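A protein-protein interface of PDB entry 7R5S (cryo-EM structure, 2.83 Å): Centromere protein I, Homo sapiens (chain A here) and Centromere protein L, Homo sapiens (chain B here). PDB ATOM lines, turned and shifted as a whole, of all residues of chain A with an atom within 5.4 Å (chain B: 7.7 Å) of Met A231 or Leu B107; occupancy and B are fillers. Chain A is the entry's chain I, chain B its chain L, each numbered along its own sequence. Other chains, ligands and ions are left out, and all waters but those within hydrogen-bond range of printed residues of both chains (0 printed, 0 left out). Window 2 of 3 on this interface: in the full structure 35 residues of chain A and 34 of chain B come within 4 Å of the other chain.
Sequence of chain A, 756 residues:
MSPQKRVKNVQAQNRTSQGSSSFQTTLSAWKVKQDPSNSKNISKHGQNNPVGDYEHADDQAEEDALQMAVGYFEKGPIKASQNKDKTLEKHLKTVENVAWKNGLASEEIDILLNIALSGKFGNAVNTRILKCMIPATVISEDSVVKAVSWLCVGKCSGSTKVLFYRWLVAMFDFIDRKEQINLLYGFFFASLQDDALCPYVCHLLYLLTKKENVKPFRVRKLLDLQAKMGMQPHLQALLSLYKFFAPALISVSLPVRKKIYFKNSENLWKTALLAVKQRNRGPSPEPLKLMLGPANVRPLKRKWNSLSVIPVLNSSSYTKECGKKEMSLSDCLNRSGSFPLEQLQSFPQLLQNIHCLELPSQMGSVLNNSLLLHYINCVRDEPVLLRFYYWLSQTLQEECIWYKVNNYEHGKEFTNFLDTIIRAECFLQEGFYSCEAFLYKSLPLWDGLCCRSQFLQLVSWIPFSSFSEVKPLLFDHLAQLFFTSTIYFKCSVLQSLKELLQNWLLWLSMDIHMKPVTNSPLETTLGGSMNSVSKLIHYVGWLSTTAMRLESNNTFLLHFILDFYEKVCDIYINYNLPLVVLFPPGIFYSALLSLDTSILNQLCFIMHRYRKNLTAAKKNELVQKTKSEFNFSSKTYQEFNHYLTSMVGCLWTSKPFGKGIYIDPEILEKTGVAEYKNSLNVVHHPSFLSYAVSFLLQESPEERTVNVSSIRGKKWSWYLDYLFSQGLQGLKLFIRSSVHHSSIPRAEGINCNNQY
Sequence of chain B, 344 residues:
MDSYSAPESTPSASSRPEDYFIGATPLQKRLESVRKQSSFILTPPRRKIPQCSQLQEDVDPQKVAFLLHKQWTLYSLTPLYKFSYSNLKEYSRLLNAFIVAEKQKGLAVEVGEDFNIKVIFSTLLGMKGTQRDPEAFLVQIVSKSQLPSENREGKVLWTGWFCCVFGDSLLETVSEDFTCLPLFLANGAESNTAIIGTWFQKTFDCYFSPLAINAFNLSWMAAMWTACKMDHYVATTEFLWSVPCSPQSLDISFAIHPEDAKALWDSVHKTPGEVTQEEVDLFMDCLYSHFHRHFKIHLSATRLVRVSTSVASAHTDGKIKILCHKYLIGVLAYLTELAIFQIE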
ATOM      1  N   GLN A 226     -15.642  17.713  19.191  1.00  0.00           N
ATOM      2  CA  GLN A 226     -16.001  16.299  19.197  1.00  0.00           C
ATOM      3  C   GLN A 226     -17.386  16.081  18.601  1.00  0.00           C
ATOM      4  O   GLN A 226     -17.611  15.109  17.872  1.00  0.00           O
ATOM      5  CB  GLN A 226     -15.941  15.745  20.621  1.00  0.00           C
ATOM      6  CG  GLN A 226     -16.385  14.296  20.737  1.00  0.00           C
ATOM      7  CD  GLN A 226     -16.733  13.903  22.157  1.00  0.00           C
ATOM      8  OE1 GLN A 226     -16.305  12.859  22.646  1.00  0.00           O
ATOM      9  NE2 GLN A 226     -17.519  14.738  22.827  1.00  0.00           N
ATOM     10  N   MET A 229     -16.921  16.444  14.735  1.00  0.00           N
ATOM     11  CA  MET A 229     -16.090  15.462  14.048  1.00  0.00           C
ATOM     12  C   MET A 229     -16.340  14.023  14.473  1.00  0.00           C
ATOM     13  O   MET A 229     -16.189  13.121  13.647  1.00  0.00           O
ATOM     14  CB  MET A 229     -14.605  15.786  14.252  1.00  0.00           C
ATOM     15  CG  MET A 229     -14.105  16.936  13.392  1.00  0.00           C
ATOM     16  SD  MET A 229     -12.330  17.206  13.535  1.00  0.00           S
ATOM     17  CE  MET A 229     -12.216  17.829  15.209  1.00  0.00           C
ATOM     18  N   GLY A 230     -16.714  13.780  15.725  1.00  0.00           N
ATOM     19  CA  GLY A 230     -16.981  12.426  16.172  1.00  0.00           C
ATOM     20  C   GLY A 230     -15.930  11.865  17.107  1.00  0.00           C
ATOM     21  O   GLY A 230     -15.279  12.613  17.841  1.00  0.00           O
ATOM     22  N   MET A 231     -15.754  10.544  17.087  1.00  0.00           N
ATOM     23  CA  MET A 231     -14.823   9.860  17.985  1.00  0.00           C
ATOM     24  C   MET A 231     -13.453   9.798  17.322  1.00  0.00           C
ATOM     25  O   MET A 231     -13.166   8.910  16.518  1.00  0.00           O
ATOM     26  CB  MET A 231     -15.333   8.467  18.334  1.00  0.00           C
ATOM     27  CG  MET A 231     -16.699   8.443  18.995  1.00  0.00           C
ATOM     28  SD  MET A 231     -17.215   6.768  19.419  1.00  0.00           S
ATOM     29  CE  MET A 231     -18.880   7.063  20.006  1.00  0.00           C
ATOM     30  N   GLN A 232     -12.592  10.751  17.669  1.00  0.00           N
ATOM     31  CA  GLN A 232     -11.227  10.776  17.172  1.00  0.00           C
ATOM     32  C   GLN A 232     -10.261  10.437  18.295  1.00  0.00           C
ATOM     33  O   GLN A 232     -10.379  11.000  19.393  1.00  0.00           O
ATOM     34  CB  GLN A 232     -10.887  12.152  16.588  1.00  0.00           C
ATOM     35  CG  GLN A 232     -11.821  12.605  15.475  1.00  0.00           C
ATOM     36  CD  GLN A 232     -11.530  11.929  14.149  1.00  0.00           C
ATOM     37  OE1 GLN A 232     -10.634  11.092  14.045  1.00  0.00           O
ATOM     38  NE2 GLN A 232     -12.291  12.291  13.123  1.00  0.00           N
ATOM     39  N   PRO A 233      -9.309   9.526  18.071  1.00  0.00           N
ATOM     40  CA  PRO A 233      -8.387   9.157  19.161  1.00  0.00           C
ATOM     41  C   PRO A 233      -7.536  10.316  19.649  1.00  0.00           C
ATOM     42  O   PRO A 233      -7.310  10.448  20.861  1.00  0.00           O
ATOM     43  CB  PRO A 233      -7.532   8.047  18.531  1.00  0.00           C
ATOM     44  CG  PRO A 233      -8.346   7.535  17.382  1.00  0.00           C
ATOM     45  CD  PRO A 233      -9.084   8.725  16.858  1.00  0.00           C
ATOM     46  N   GLN A 236      -9.830  11.983  21.890  1.00  0.00           N
ATOM     47  CA  GLN A 236     -10.149  11.214  23.089  1.00  0.00           C
ATOM     48  C   GLN A 236      -9.019  11.285  24.107  1.00  0.00           C
ATOM     49  O   GLN A 236      -9.268  11.376  25.315  1.00  0.00           O
ATOM     50  CB  GLN A 236     -10.446   9.762  22.719  1.00  0.00           C
ATOM     51  CG  GLN A 236     -11.772   9.561  22.007  1.00  0.00           C
ATOM     52  CD  GLN A 236     -12.041   8.106  21.681  1.00  0.00           C
ATOM     53  OE1 GLN A 236     -11.132   7.277  21.696  1.00  0.00           O
ATOM     54  NE2 GLN A 236     -13.295   7.788  21.382  1.00  0.00           N
ATOM     55  N   SER A 251     -16.579  14.297  32.332  1.00  0.00           N
ATOM     56  CA  SER A 251     -16.707  12.892  32.710  1.00  0.00           C
ATOM     57  C   SER A 251     -16.533  12.043  31.458  1.00  0.00           C
ATOM     58  O   SER A 251     -17.370  12.091  30.549  1.00  0.00           O
ATOM     59  CB  SER A 251     -18.056  12.625  33.375  1.00  0.00           C
ATOM     60  OG  SER A 251     -18.032  11.409  34.100  1.00  0.00           O
ATOM     61  N   VAL A 252     -15.452  11.268  31.410  1.00  0.00           N
ATOM     62  CA  VAL A 252     -15.117  10.442  30.255  1.00  0.00           C
ATOM     63  C   VAL A 252     -14.678   9.068  30.743  1.00  0.00           C
ATOM     64  O   VAL A 252     -13.869   8.957  31.670  1.00  0.00           O
ATOM     65  CB  VAL A 252     -14.009  11.088  29.394  1.00  0.00           C
ATOM     66  CG1 VAL A 252     -13.524  10.121  28.328  1.00  0.00           C
ATOM     67  CG2 VAL A 252     -14.506  12.368  28.755  1.00  0.00           C
ATOM     68  N   VAL B 100     -24.274   9.036  33.016  1.00  0.00           N
ATOM     69  CA  VAL B 100     -24.462   9.325  31.596  1.00  0.00           C
ATOM     70  C   VAL B 100     -23.185   9.032  30.818  1.00  0.00           C
ATOM     71  O   VAL B 100     -23.230   8.485  29.710  1.00  0.00           O
ATOM     72  CB  VAL B 100     -24.933  10.778  31.403  1.00  0.00           C
ATOM     73  CG1 VAL B 100     -24.903  11.159  29.934  1.00  0.00           C
ATOM     74  CG2 VAL B 100     -26.333  10.951  31.963  1.00  0.00           C
ATOM     75  N   ALA B 101     -22.026   9.376  31.388  1.00  0.00           N
ATOM     76  CA  ALA B 101     -20.766   9.074  30.718  1.00  0.00           C
ATOM     77  C   ALA B 101     -20.501   7.575  30.666  1.00  0.00           C
ATOM     78  O   ALA B 101     -19.850   7.094  29.731  1.00  0.00           O
ATOM     79  CB  ALA B 101     -19.612   9.793  31.415  1.00  0.00           C
ATOM     80  N   GLU B 102     -20.993   6.824  31.652  1.00  0.00           N
ATOM     81  CA  GLU B 102     -20.822   5.376  31.643  1.00  0.00           C
ATOM     82  C   GLU B 102     -21.770   4.698  30.662  1.00  0.00           C
ATOM     83  O   GLU B 102     -21.452   3.619  30.149  1.00  0.00           O
ATOM     84  CB  GLU B 102     -21.035   4.814  33.049  1.00  0.00           C
ATOM     85  CG  GLU B 102     -20.478   3.415  33.255  1.00  0.00           C
ATOM     86  CD  GLU B 102     -18.973   3.407  33.440  1.00  0.00           C
ATOM     87  OE1 GLU B 102     -18.393   4.490  33.667  1.00  0.00           O
ATOM     88  OE2 GLU B 102     -18.370   2.316  33.360  1.00  0.00           O
ATOM     89  N   GLN B 104     -22.828   5.865  27.563  1.00  0.00           N
ATOM     90  CA  GLN B 104     -22.218   5.992  26.241  1.00  0.00           C
ATOM     91  C   GLN B 104     -20.704   5.984  26.430  1.00  0.00           C
ATOM     92  O   GLN B 104     -20.111   6.986  26.836  1.00  0.00           O
ATOM     93  CB  GLN B 104     -22.698   7.255  25.527  1.00  0.00           C
ATOM     94  CG  GLN B 104     -22.895   8.469  26.425  1.00  0.00           C
ATOM     95  CD  GLN B 104     -23.434   9.670  25.667  1.00  0.00           C
ATOM     96  OE1 GLN B 104     -23.736   9.581  24.476  1.00  0.00           O
ATOM     97  NE2 GLN B 104     -23.564  10.798  26.355  1.00  0.00           N
ATOM     98  N   LYS B 105     -20.083   4.848  26.125  1.00  0.00           N
ATOM     99  CA  LYS B 105     -18.666   4.636  26.389  1.00  0.00           C
ATOM    100  C   LYS B 105     -17.755   5.400  25.435  1.00  0.00           C
ATOM    101  O   LYS B 105     -16.533   5.388  25.625  1.00  0.00           O
ATOM    102  CB  LYS B 105     -18.358   3.136  26.317  1.00  0.00           C
ATOM    103  CG  LYS B 105     -17.056   2.710  26.975  1.00  0.00           C
ATOM    104  CD  LYS B 105     -17.086   2.942  28.478  1.00  0.00           C
ATOM    105  CE  LYS B 105     -18.308   2.301  29.120  1.00  0.00           C
ATOM    106  NZ  LYS B 105     -18.045   1.920  30.533  1.00  0.00           N
ATOM    107  N   GLY B 106     -18.305   6.072  24.428  1.00  0.00           N
ATOM    108  CA  GLY B 106     -17.479   6.703  23.419  1.00  0.00           C
ATOM    109  C   GLY B 106     -17.214   8.182  23.610  1.00  0.00           C
ATOM    110  O   GLY B 106     -16.064   8.625  23.521  1.00  0.00           O
ATOM    111  N   LEU B 107     -18.260   8.958  23.874  1.00  0.00           N
ATOM    112  CA  LEU B 107     -18.171  10.409  23.849  1.00  0.00           C
ATOM    113  C   LEU B 107     -18.054  10.988  25.254  1.00  0.00           C
ATOM    114  O   LEU B 107     -18.304  10.317  26.258  1.00  0.00           O
ATOM    115  CB  LEU B 107     -19.388  11.011  23.141  1.00  0.00           C
ATOM    116  CG  LEU B 107     -19.761  10.413  21.783  1.00  0.00           C
ATOM    117  CD1 LEU B 107     -20.915   9.433  21.924  1.00  0.00           C
ATOM    118  CD2 LEU B 107     -20.100  11.511  20.788  1.00  0.00           C
ATOM    119  N   ALA B 108     -17.666  12.260  25.305  1.00  0.00           N
ATOM    120  CA  ALA B 108     -17.545  12.993  26.551  1.00  0.00           C
ATOM    121  C   ALA B 108     -18.906  13.526  26.992  1.00  0.00           C
ATOM    122  O   ALA B 108     -19.870  13.568  26.223  1.00  0.00           O
ATOM    123  CB  ALA B 108     -16.548  14.141  26.400  1.00  0.00           C
ATOM    124  N   VAL B 109     -18.976  13.943  28.253  1.00  0.00           N
ATOM    125  CA  VAL B 109     -20.221  14.414  28.853  1.00  0.00           C
ATOM    126  C   VAL B 109     -19.900  15.565  29.795  1.00  0.00           C
ATOM    127  O   VAL B 109     -18.992  15.462  30.626  1.00  0.00           O
ATOM    128  CB  VAL B 109     -20.955  13.278  29.596  1.00  0.00           C
ATOM    129  CG1 VAL B 109     -21.897  13.841  30.646  1.00  0.00           C
ATOM    130  CG2 VAL B 109     -21.716  12.405  28.615  1.00  0.00           C
ATOM    131  N   GLU B 110     -20.641  16.661  29.663  1.00  0.00           N
ATOM    132  CA  GLU B 110     -20.480  17.796  30.557  1.00  0.00           C
ATOM    133  C   GLU B 110     -21.285  17.582  31.838  1.00  0.00           C
ATOM    134  O   GLU B 110     -22.255  16.821  31.875  1.00  0.00           O
ATOM    135  CB  GLU B 110     -20.915  19.090  29.867  1.00  0.00           C
ATOM    136  CG  GLU B 110     -20.258  20.342  30.422  1.00  0.00           C
ATOM    137  CD  GLU B 110     -20.583  21.578  29.609  1.00  0.00           C
ATOM    138  OE1 GLU B 110     -21.522  21.521  28.788  1.00  0.00           O
ATOM    139  OE2 GLU B 110     -19.898  22.607  29.790  1.00  0.00           O
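The backbone NH of Ala B108 is in hydrogen-bond range of the side-chain amide oxygen of Gln A226 (3.0 Å).
The backbone NH of Ser A251 lies within hydrogen-bond range of the backbone carbonyl oxygen of Val B109 (3.2 Å).
OE1 of Gln A226 touches CA of Leu B107 (3.3 Å).
Gly B106 touches Met A231 (CA to CE, 3.7 Å).
Leu B107 touches Met A231 (CD1 to CE, 3.7 Å).
Gln A236 touches Gly B106.
CB of Ala B101 touches O of Ser A251, 3.3 Å away.
Val A252 touches Ala B108.
Met A231 touches just these residues of chain B: Gly B106 and Leu B107.
Leu B107 touches just these residues of chain A: Gln A226 (3.3 Å) and Met A231 (3.7 Å).
Printed residues of chain B within 4 Å of Val A252: Ala B108.
Of the printed residues of chain B, Gln A236 touches Gly B106.
Of the printed residues of chain B, Ser A251 touches Ala B101 and Val B109.
Val B100 touches none of the printed residues of chain A.
Gln A232 touches none of the printed residues of chain B.
The nearest residue of chain B that does not touch Met A231 is Lys B105 (5.8 Å).
The nearest printed residue of chain A that does not touch Val B109 is Val A252 (4.8 Å).
Hydrophobic or aromatic side chains of chain B within 4 Å of the printed part of chain A: Ala B101, Leu B107, Ala B108 and Val B109.
Printed residues of chain A that touch a printed residue of chain B: Gln A226, Met A231, Gln A236, Ser A251 and Val A252.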
